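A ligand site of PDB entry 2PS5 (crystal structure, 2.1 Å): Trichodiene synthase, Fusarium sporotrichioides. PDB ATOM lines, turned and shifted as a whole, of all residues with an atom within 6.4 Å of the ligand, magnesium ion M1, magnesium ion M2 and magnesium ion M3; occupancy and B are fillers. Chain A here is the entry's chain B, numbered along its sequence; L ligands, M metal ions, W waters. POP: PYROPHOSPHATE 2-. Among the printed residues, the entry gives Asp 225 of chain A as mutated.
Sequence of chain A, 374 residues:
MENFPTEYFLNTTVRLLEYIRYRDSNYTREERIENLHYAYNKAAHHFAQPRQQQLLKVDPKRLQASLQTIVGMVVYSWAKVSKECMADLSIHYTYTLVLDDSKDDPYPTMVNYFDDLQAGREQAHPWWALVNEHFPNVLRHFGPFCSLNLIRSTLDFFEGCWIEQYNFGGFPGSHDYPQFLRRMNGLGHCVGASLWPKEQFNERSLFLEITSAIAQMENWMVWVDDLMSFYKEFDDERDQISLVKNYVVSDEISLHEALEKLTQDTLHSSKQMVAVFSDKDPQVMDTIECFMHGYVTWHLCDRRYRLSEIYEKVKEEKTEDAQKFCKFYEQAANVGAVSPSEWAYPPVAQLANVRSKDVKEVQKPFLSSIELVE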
ATOM      1  N   LEU A  97      -1.222  12.478 -22.683  1.00  0.00           N
ATOM      2  CA  LEU A  97      -1.518  13.908 -22.727  1.00  0.00           C
ATOM      3  C   LEU A  97      -0.378  14.673 -22.073  1.00  0.00           C
ATOM      4  O   LEU A  97      -0.015  15.773 -22.514  1.00  0.00           O
ATOM      5  CB  LEU A  97      -2.815  14.244 -21.979  1.00  0.00           C
ATOM      6  CG  LEU A  97      -3.370  15.640 -22.301  1.00  0.00           C
ATOM      7  CD1 LEU A  97      -3.921  15.626 -23.721  1.00  0.00           C
ATOM      8  CD2 LEU A  97      -4.476  16.044 -21.332  1.00  0.00           C
ATOM      9  N   ASP A 100       2.192  14.869 -24.490  1.00  0.00           N
ATOM     10  CA  ASP A 100       1.649  15.713 -25.547  1.00  0.00           C
ATOM     11  C   ASP A 100       1.975  17.205 -25.444  1.00  0.00           C
ATOM     12  O   ASP A 100       2.160  17.873 -26.467  1.00  0.00           O
ATOM     13  CB  ASP A 100       0.131  15.537 -25.623  1.00  0.00           C
ATOM     14  CG  ASP A 100      -0.463  16.153 -26.871  1.00  0.00           C
ATOM     15  OD1 ASP A 100      -0.257  15.581 -27.957  1.00  0.00           O
ATOM     16  OD2 ASP A 100      -1.128  17.207 -26.769  1.00  0.00           O
ATOM     17  N   ASP A 101       2.030  17.727 -24.229  1.00  0.00           N
ATOM     18  CA  ASP A 101       2.328  19.150 -24.035  1.00  0.00           C
ATOM     19  C   ASP A 101       3.744  19.339 -23.508  1.00  0.00           C
ATOM     20  O   ASP A 101       4.198  20.462 -23.306  1.00  0.00           O
ATOM     21  CB  ASP A 101       1.359  19.778 -23.029  1.00  0.00           C
ATOM     22  CG  ASP A 101      -0.089  19.663 -23.434  1.00  0.00           C
ATOM     23  OD1 ASP A 101      -0.410  19.938 -24.626  1.00  0.00           O
ATOM     24  OD2 ASP A 101      -0.922  19.327 -22.574  1.00  0.00           O
ATOM     25  N   PHE A 157       2.975   7.506 -31.319  1.00  0.00           N
ATOM     26  CA  PHE A 157       2.716   8.736 -30.595  1.00  0.00           C
ATOM     27  C   PHE A 157       4.015   9.279 -30.009  1.00  0.00           C
ATOM     28  O   PHE A 157       4.274  10.479 -30.088  1.00  0.00           O
ATOM     29  CB  PHE A 157       1.700   8.473 -29.481  1.00  0.00           C
ATOM     30  CG  PHE A 157       1.438   9.669 -28.618  1.00  0.00           C
ATOM     31  CD1 PHE A 157       0.703  10.739 -29.099  1.00  0.00           C
ATOM     32  CD2 PHE A 157       1.958   9.732 -27.326  1.00  0.00           C
ATOM     33  CE1 PHE A 157       0.490  11.867 -28.301  1.00  0.00           C
ATOM     34  CE2 PHE A 157       1.747  10.843 -26.523  1.00  0.00           C
ATOM     35  CZ  PHE A 157       1.006  11.913 -27.021  1.00  0.00           C
ATOM     36  N   CYS A 161       5.643  13.034 -30.804  1.00  0.00           N
ATOM     37  CA  CYS A 161       6.010  14.113 -29.880  1.00  0.00           C
ATOM     38  C   CYS A 161       7.496  14.479 -30.060  1.00  0.00           C
ATOM     39  O   CYS A 161       7.892  15.630 -29.857  1.00  0.00           O
ATOM     40  CB  CYS A 161       5.735  13.682 -28.428  1.00  0.00           C
ATOM     41  SG  CYS A 161       3.978  13.339 -28.030  1.00  0.00           S
ATOM     42  N   GLU A 164       7.720  16.760 -33.071  1.00  0.00           N
ATOM     43  CA  GLU A 164       7.171  18.074 -32.744  1.00  0.00           C
ATOM     44  C   GLU A 164       8.163  18.928 -31.961  1.00  0.00           C
ATOM     45  O   GLU A 164       8.091  20.164 -32.015  1.00  0.00           O
ATOM     46  CB  GLU A 164       5.856  17.928 -31.963  1.00  0.00           C
ATOM     47  CG  GLU A 164       4.794  17.139 -32.721  1.00  0.00           C
ATOM     48  CD  GLU A 164       3.480  16.998 -31.965  1.00  0.00           C
ATOM     49  OE1 GLU A 164       3.484  16.888 -30.723  1.00  0.00           O
ATOM     50  OE2 GLU A 164       2.423  16.997 -32.634  1.00  0.00           O
ATOM     51  N   ARG A 182       0.384  13.941 -38.410  1.00  0.00           N
ATOM     52  CA  ARG A 182      -0.882  13.854 -37.697  1.00  0.00           C
ATOM     53  C   ARG A 182      -1.229  12.403 -37.332  1.00  0.00           C
ATOM     54  O   ARG A 182      -1.700  12.148 -36.231  1.00  0.00           O
ATOM     55  CB  ARG A 182      -2.004  14.486 -38.526  1.00  0.00           C
ATOM     56  CG  ARG A 182      -3.332  14.639 -37.773  1.00  0.00           C
ATOM     57  CD  ARG A 182      -3.106  15.090 -36.329  1.00  0.00           C
ATOM     58  NE  ARG A 182      -4.360  15.507 -35.695  1.00  0.00           N
ATOM     59  CZ  ARG A 182      -4.527  15.619 -34.381  1.00  0.00           C
ATOM     60  NH1 ARG A 182      -3.538  15.344 -33.542  1.00  0.00           N
ATOM     61  NH2 ARG A 182      -5.706  16.013 -33.904  1.00  0.00           N
ATOM     62  N   ASN A 185       1.162  11.358 -34.511  1.00  0.00           N
ATOM     63  CA  ASN A 185       0.806  11.838 -33.181  1.00  0.00           C
ATOM     64  C   ASN A 185      -0.665  11.702 -32.781  1.00  0.00           C
ATOM     65  O   ASN A 185      -1.044  12.035 -31.660  1.00  0.00           O
ATOM     66  CB  ASN A 185       1.206  13.321 -33.005  1.00  0.00           C
ATOM     67  CG  ASN A 185       0.375  14.258 -33.884  1.00  0.00           C
ATOM     68  OD1 ASN A 185      -0.815  14.035 -34.112  1.00  0.00           O
ATOM     69  ND2 ASN A 185       1.009  15.342 -34.356  1.00  0.00           N
ATOM     70  N   GLY A 186      -1.501  11.200 -33.697  1.00  0.00           N
ATOM     71  CA  GLY A 186      -2.921  11.104 -33.427  1.00  0.00           C
ATOM     72  C   GLY A 186      -3.491  10.035 -32.520  1.00  0.00           C
ATOM     73  O   GLY A 186      -4.642  10.146 -32.115  1.00  0.00           O
ATOM     74  N   VAL A 222      -8.958  12.275 -35.378  1.00  0.00           N
ATOM     75  CA  VAL A 222      -7.942  13.314 -35.475  1.00  0.00           C
ATOM     76  C   VAL A 222      -8.435  14.576 -36.165  1.00  0.00           C
ATOM     77  O   VAL A 222      -8.168  15.683 -35.705  1.00  0.00           O
ATOM     78  CB  VAL A 222      -6.656  12.802 -36.201  1.00  0.00           C
ATOM     79  CG1 VAL A 222      -6.023  11.674 -35.400  1.00  0.00           C
ATOM     80  CG2 VAL A 222      -6.970  12.344 -37.618  1.00  0.00           C
ATOM     81  N   ASP A 225     -10.731  16.628 -33.968  1.00  0.00           N
ATOM     82  CA  ASP A 225      -9.987  17.351 -32.937  1.00  0.00           C
ATOM     83  C   ASP A 225      -9.208  18.505 -33.550  1.00  0.00           C
ATOM     84  O   ASP A 225      -9.066  19.565 -32.937  1.00  0.00           O
ATOM     85  CB  ASP A 225      -9.038  16.428 -32.179  1.00  0.00           C
ATOM     86  CG  ASP A 225      -8.148  17.192 -31.211  1.00  0.00           C
ATOM     87  OD1 ASP A 225      -7.021  17.574 -31.593  1.00  0.00           O
ATOM     88  OD2 ASP A 225      -8.592  17.426 -30.066  1.00  0.00           O
ATOM     89  N   ASP A 226      -8.698  18.321 -34.755  1.00  0.00           N
ATOM     90  CA  ASP A 226      -7.946  19.387 -35.392  1.00  0.00           C
ATOM     91  C   ASP A 226      -8.864  20.599 -35.557  1.00  0.00           C
ATOM     92  O   ASP A 226      -8.487  21.730 -35.246  1.00  0.00           O
ATOM     93  CB  ASP A 226      -7.422  18.922 -36.756  1.00  0.00           C
ATOM     94  CG  ASP A 226      -6.115  18.150 -36.637  1.00  0.00           C
ATOM     95  OD1 ASP A 226      -5.248  18.598 -35.871  1.00  0.00           O
ATOM     96  OD2 ASP A 226      -5.951  17.105 -37.320  1.00  0.00           O
ATOM     97  N   SER A 229     -10.220  21.822 -31.822  1.00  0.00           N
ATOM     98  CA  SER A 229      -9.169  22.303 -30.925  1.00  0.00           C
ATOM     99  C   SER A 229      -8.359  23.403 -31.597  1.00  0.00           C
ATOM    100  O   SER A 229      -7.309  23.811 -31.095  1.00  0.00           O
ATOM    101  CB  SER A 229      -8.236  21.165 -30.514  1.00  0.00           C
ATOM    102  OG  SER A 229      -7.258  20.905 -31.511  1.00  0.00           O
ATOM    103  N   PHE A 230      -8.851  23.889 -32.735  1.00  0.00           N
ATOM    104  CA  PHE A 230      -8.174  24.933 -33.488  1.00  0.00           C
ATOM    105  C   PHE A 230      -8.000  26.196 -32.643  1.00  0.00           C
ATOM    106  O   PHE A 230      -6.950  26.844 -32.679  1.00  0.00           O
ATOM    107  CB  PHE A 230      -8.976  25.255 -34.753  1.00  0.00           C
ATOM    108  CG  PHE A 230      -8.363  26.320 -35.618  1.00  0.00           C
ATOM    109  CD1 PHE A 230      -6.988  26.341 -35.853  1.00  0.00           C
ATOM    110  CD2 PHE A 230      -9.154  27.296 -36.212  1.00  0.00           C
ATOM    111  CE1 PHE A 230      -6.408  27.318 -36.669  1.00  0.00           C
ATOM    112  CE2 PHE A 230      -8.588  28.274 -37.024  1.00  0.00           C
ATOM    113  CZ  PHE A 230      -7.207  28.282 -37.261  1.00  0.00           C
ATOM    114  N   LYS A 232      -7.830  26.690 -29.117  1.00  0.00           N
ATOM    115  CA  LYS A 232      -6.811  26.627 -28.057  1.00  0.00           C
ATOM    116  C   LYS A 232      -5.377  26.447 -28.565  1.00  0.00           C
ATOM    117  O   LYS A 232      -4.426  26.781 -27.865  1.00  0.00           O
ATOM    118  CB  LYS A 232      -7.149  25.530 -27.043  1.00  0.00           C
ATOM    119  CG  LYS A 232      -6.876  24.092 -27.494  1.00  0.00           C
ATOM    120  CD  LYS A 232      -5.422  23.664 -27.229  1.00  0.00           C
ATOM    121  CE  LYS A 232      -5.213  22.187 -27.546  1.00  0.00           C
ATOM    122  NZ  LYS A 232      -3.824  21.714 -27.244  1.00  0.00           N
ATOM    123  N   GLU A 233      -5.231  25.917 -29.777  1.00  0.00           N
ATOM    124  CA  GLU A 233      -3.902  25.700 -30.350  1.00  0.00           C
ATOM    125  C   GLU A 233      -3.391  26.914 -31.118  1.00  0.00           C
ATOM    126  O   GLU A 233      -2.195  27.196 -31.120  1.00  0.00           O
ATOM    127  CB  GLU A 233      -3.925  24.486 -31.288  1.00  0.00           C
ATOM    128  CG  GLU A 233      -4.341  23.174 -30.649  1.00  0.00           C
ATOM    129  CD  GLU A 233      -4.226  21.992 -31.581  1.00  0.00           C
ATOM    130  OE1 GLU A 233      -4.756  22.071 -32.715  1.00  0.00           O
ATOM    131  OE2 GLU A 233      -3.618  20.981 -31.186  1.00  0.00           O
ATOM    132  N   ARG A 238       3.434  25.673 -28.113  1.00  0.00           N
ATOM    133  CA  ARG A 238       3.582  24.234 -28.229  1.00  0.00           C
ATOM    134  C   ARG A 238       2.765  23.623 -29.373  1.00  0.00           C
ATOM    135  O   ARG A 238       3.119  22.582 -29.922  1.00  0.00           O
ATOM    136  CB  ARG A 238       3.185  23.555 -26.910  1.00  0.00           C
ATOM    137  CG  ARG A 238       2.959  22.052 -27.002  1.00  0.00           C
ATOM    138  CD  ARG A 238       4.225  21.309 -27.372  1.00  0.00           C
ATOM    139  NE  ARG A 238       3.938  19.958 -27.852  1.00  0.00           N
ATOM    140  CZ  ARG A 238       4.860  19.037 -28.102  1.00  0.00           C
ATOM    141  NH1 ARG A 238       6.139  19.325 -27.911  1.00  0.00           N
ATOM    142  NH2 ARG A 238       4.501  17.833 -28.530  1.00  0.00           N
ATOM    143  N   ASP A 239       1.675  24.292 -29.750  1.00  0.00           N
ATOM    144  CA  ASP A 239       0.818  23.781 -30.806  1.00  0.00           C
ATOM    145  C   ASP A 239       0.925  24.486 -32.154  1.00  0.00           C
ATOM    146  O   ASP A 239       0.077  24.279 -33.021  1.00  0.00           O
ATOM    147  CB  ASP A 239      -0.647  23.787 -30.342  1.00  0.00           C
ATOM    148  CG  ASP A 239      -0.839  23.164 -28.971  1.00  0.00           C
ATOM    149  OD1 ASP A 239      -0.010  22.299 -28.585  1.00  0.00           O
ATOM    150  OD2 ASP A 239      -1.826  23.514 -28.277  1.00  0.00           O
ATOM    151  N   TRP A 298     -17.325  16.310 -25.313  1.00  0.00           N
ATOM    152  CA  TRP A 298     -16.114  16.550 -24.546  1.00  0.00           C
ATOM    153  C   TRP A 298     -15.345  17.785 -25.020  1.00  0.00           C
ATOM    154  O   TRP A 298     -14.856  18.575 -24.197  1.00  0.00           O
ATOM    155  CB  TRP A 298     -15.223  15.302 -24.603  1.00  0.00           C
ATOM    156  CG  TRP A 298     -13.895  15.495 -23.977  1.00  0.00           C
ATOM    157  CD1 TRP A 298     -13.623  15.777 -22.667  1.00  0.00           C
ATOM    158  CD2 TRP A 298     -12.626  15.385 -24.643  1.00  0.00           C
ATOM    159  NE1 TRP A 298     -12.265  15.847 -22.466  1.00  0.00           N
ATOM    160  CE2 TRP A 298     -11.630  15.610 -23.664  1.00  0.00           C
ATOM    161  CE3 TRP A 298     -12.231  15.111 -25.960  1.00  0.00           C
ATOM    162  CZ2 TRP A 298     -10.259  15.571 -23.971  1.00  0.00           C
ATOM    163  CZ3 TRP A 298     -10.874  15.073 -26.264  1.00  0.00           C
ATOM    164  CH2 TRP A 298      -9.895  15.303 -25.268  1.00  0.00           C
ATOM    165  N   HIS A 299     -15.234  17.962 -26.331  1.00  0.00           N
ATOM    166  CA  HIS A 299     -14.538  19.109 -26.900  1.00  0.00           C
ATOM    167  C   HIS A 299     -15.243  20.432 -26.596  1.00  0.00           C
ATOM    168  O   HIS A 299     -14.594  21.475 -26.445  1.00  0.00           O
ATOM    169  CB  HIS A 299     -14.390  18.951 -28.409  1.00  0.00           C
ATOM    170  CG  HIS A 299     -13.278  18.037 -28.815  1.00  0.00           C
ATOM    171  ND1 HIS A 299     -11.950  18.392 -28.740  1.00  0.00           N
ATOM    172  CD2 HIS A 299     -13.294  16.751 -29.244  1.00  0.00           C
ATOM    173  CE1 HIS A 299     -11.198  17.382 -29.116  1.00  0.00           C
ATOM    174  NE2 HIS A 299     -11.986  16.366 -29.428  1.00  0.00           N
ATOM    175  N   ARG A 304      -9.631  22.430 -21.423  1.00  0.00           N
ATOM    176  CA  ARG A 304      -8.524  22.383 -22.381  1.00  0.00           C
ATOM    177  C   ARG A 304      -8.799  23.070 -23.713  1.00  0.00           C
ATOM    178  O   ARG A 304      -7.918  23.731 -24.270  1.00  0.00           O
ATOM    179  CB  ARG A 304      -8.123  20.921 -22.636  1.00  0.00           C
ATOM    180  CG  ARG A 304      -6.894  20.747 -23.534  1.00  0.00           C
ATOM    181  CD  ARG A 304      -6.623  19.274 -23.846  1.00  0.00           C
ATOM    182  NE  ARG A 304      -5.425  19.072 -24.674  1.00  0.00           N
ATOM    183  CZ  ARG A 304      -4.167  19.161 -24.229  1.00  0.00           C
ATOM    184  NH1 ARG A 304      -3.928  19.450 -22.951  1.00  0.00           N
ATOM    185  NH2 ARG A 304      -3.147  18.945 -25.056  1.00  0.00           N
ATOM    186  N   TYR A 305     -10.016  22.934 -24.233  1.00  0.00           N
ATOM    187  CA  TYR A 305     -10.337  23.522 -25.530  1.00  0.00           C
ATOM    188  C   TYR A 305     -10.896  24.943 -25.511  1.00  0.00           C
ATOM    189  O   TYR A 305     -11.154  25.540 -26.561  1.00  0.00           O
ATOM    190  CB  TYR A 305     -11.253  22.565 -26.285  1.00  0.00           C
ATOM    191  CG  TYR A 305     -10.568  21.229 -26.438  1.00  0.00           C
ATOM    192  CD1 TYR A 305      -9.384  21.120 -27.162  1.00  0.00           C
ATOM    193  CD2 TYR A 305     -11.021  20.098 -25.758  1.00  0.00           C
ATOM    194  CE1 TYR A 305      -8.660  19.939 -27.195  1.00  0.00           C
ATOM    195  CE2 TYR A 305     -10.310  18.902 -25.781  1.00  0.00           C
ATOM    196  CZ  TYR A 305      -9.128  18.838 -26.497  1.00  0.00           C
ATOM    197  OH  TYR A 305      -8.382  17.684 -26.487  1.00  0.00           O
HETATM  198  P1  POP L   1      -3.471  16.833 -30.267  1.00  0.00           P
HETATM  199  O1  POP L   1      -3.965  17.720 -31.386  1.00  0.00           O
HETATM  200  O2  POP L   1      -2.039  17.131 -29.991  1.00  0.00           O
HETATM  201  O3  POP L   1      -3.635  15.374 -30.570  1.00  0.00           O
HETATM  202  O   POP L   1      -4.585  16.960 -29.062  1.00  0.00           O
HETATM  203  P2  POP L   1      -4.978  18.336 -28.225  1.00  0.00           P
HETATM  204  O4  POP L   1      -5.595  19.404 -29.179  1.00  0.00           O
HETATM  205  O5  POP L   1      -3.690  18.810 -27.589  1.00  0.00           O
HETATM  206  O6  POP L   1      -5.980  17.829 -27.305  1.00  0.00           O
HETATM  207 MG    MG M   1      -5.523  19.296 -31.389  1.00  0.00          MG
HETATM  208 MG    MG M   2      -1.513  18.507 -28.447  1.00  0.00          MG
HETATM  209 MG    MG M   3      -0.210  16.120 -30.079  1.00  0.00          MG
HETATM  210  O   HOH W   1      -2.753  13.812 -27.664  1.00  0.00           O
HETATM  211  O   HOH W   2      -1.184  14.277 -30.389  1.00  0.00           O
HETATM  212  O   HOH W   3       1.092  20.026 -30.193  1.00  0.00           O
HETATM  213  O   HOH W   4      -1.738  19.985 -29.765  1.00  0.00           O
HETATM  214  O   HOH W   5       1.738  15.282 -29.799  1.00  0.00           O
HETATM  215  O   HOH W   6      -1.927  18.531 -32.989  1.00  0.00           O
HETATM  216  O   HOH W   7       0.849  18.118 -28.561  1.00  0.00           O
HETATM  217  O   HOH W   8      -0.872  19.991 -27.245  1.00  0.00           O
HETATM  218  O   HOH W   9      -5.233  19.606 -33.406  1.00  0.00           O
HETATM  219  O   HOH W  10      -0.142  17.121 -31.938  1.00  0.00           O
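The side-chain hydroxyl (OH) of Tyr 305 is in hydrogen-bond range of an oxygen (O6) of the ligand (2.5 Å).
NE of Arg 304 lies within salt-bridge range of O6 of the ligand (3.0 Å).
An oxygen (O5) of the ligand sits close to the side-chain amino group (NZ) of Lys 232, at 2.9 Å.
NH1 of Arg 182 lies within salt-bridge range of O3 of the ligand (3.0 Å).
Magnesium ion M1 is bound by water W9 (2.1 Å), O4 of the ligand (2.2 Å), O1 of the ligand (2.2 Å), OD1 of Asp 225 (2.3 Å), OG of Ser 229 (2.4 Å) and OE2 of Glu 233 (2.6 Å).
Magnesium ion M1 has six donor atoms within binding distance.
Within 4 Å of magnesium ion M1: Asp 225, Ser 229 and Glu 233.
NH2 of Arg 304 touches magnesium ion M2 (3.8 Å).
Two residues have an atom within 4 Å of magnesium ion M2: Asp 100 and Arg 304.
The nearest printed residue that does not touch magnesium ion M2 is Asp 239 (4.1 Å).
Magnesium ion M2 is bound by water W4 (2.0 Å), water W8 (2.0 Å), O2 of the ligand (2.1 Å), OD2 of Asp 100 (2.2 Å), O5 of the ligand (2.4 Å) and water W7 (2.4 Å).
Magnesium ion M2 has six donor atoms within binding distance.
Residues that only touch magnesium ion M3: Glu 164 (3.8 Å).
Two residues have an atom within 4 Å of magnesium ion M3: Asp 100 and Glu 164.
The nearest printed residue that does not touch magnesium ion M3 is Asn 185 (4.3 Å).
Hydrophobic or aromatic side chains that line the ligand: Tyr 305.
Of the 22 residues printed, 8 come within 4 Å of the ligand.
The nearest printed residue that does not touch the ligand is Asn 185 (4.4 Å).
Water W9 bridges OE1 of Glu 233 (2.6 Å) and OD1 of Asp 226 (2.7 Å).
Water W8 lies within hydrogen-bond range of the side-chain carboxylate (OD1) of Asp 101 (2.7 Å), the side-chain carboxylate (OD1) of Asp 239 (2.8 Å), the guanidinium group (NH2) of Arg 304 (3.3 Å) and the side-chain amino group (NZ) of Lys 232 (3.4 Å).
Water W10 lies within hydrogen-bond range of OE2 of Glu 164 (2.7 Å) and ND2 of Asn 185 (3.2 Å).
Water W5 lies within hydrogen-bond range of OE1 of Glu 164 (2.5 Å) and SG of Cys 161 (3.5 Å).
Water W2 bridges O of Asn 185 (2.6 Å) and O3 of the ligand (2.7 Å).
Water W3 lies within hydrogen-bond range of OD1 of Asp 239 (3.0 Å) and O of Arg 238 (3.3 Å).
Magnesium ion M3 is bound by O2 of the ligand (2.1 Å), water W2 (2.1 Å), water W10 (2.1 Å), water W5 (2.1 Å) and OD1 of Asp 100 (2.2 Å).
Slightly farther from magnesium ion M3 lies water W7 (2.7 Å).
OD2 of Asp 100 lies close to NH2 of Arg 304, at 3.2 Å.
The guanidinium group (NE) of Arg 238 sits at hydrogen-bond distance from the backbone carbonyl oxygen (O) of Asp 100.
NH2 of Arg 182 lies close to OD1 of Asp 225, 3.1 Å away.
The guanidinium group (NH2) of Arg 304 is in salt-bridge range of the side-chain carboxylate (OD1) of Asp 101.
The side-chain amino group of Lys 232 lies within salt-bridge range of the side-chain carboxylate of Asp 239 (2.9 Å).
NE of Arg 182 lies within salt-bridge range of OD2 of Asp 226, 2.8 Å away.
The backbone carbonyl oxygen (O) of Val 222 lies within hydrogen-bond range of the guanidinium group (NH2) of Arg 182.
OE2 of Glu 164 is in hydrogen-bond range of ND2 of Asn 185 (2.8 Å).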
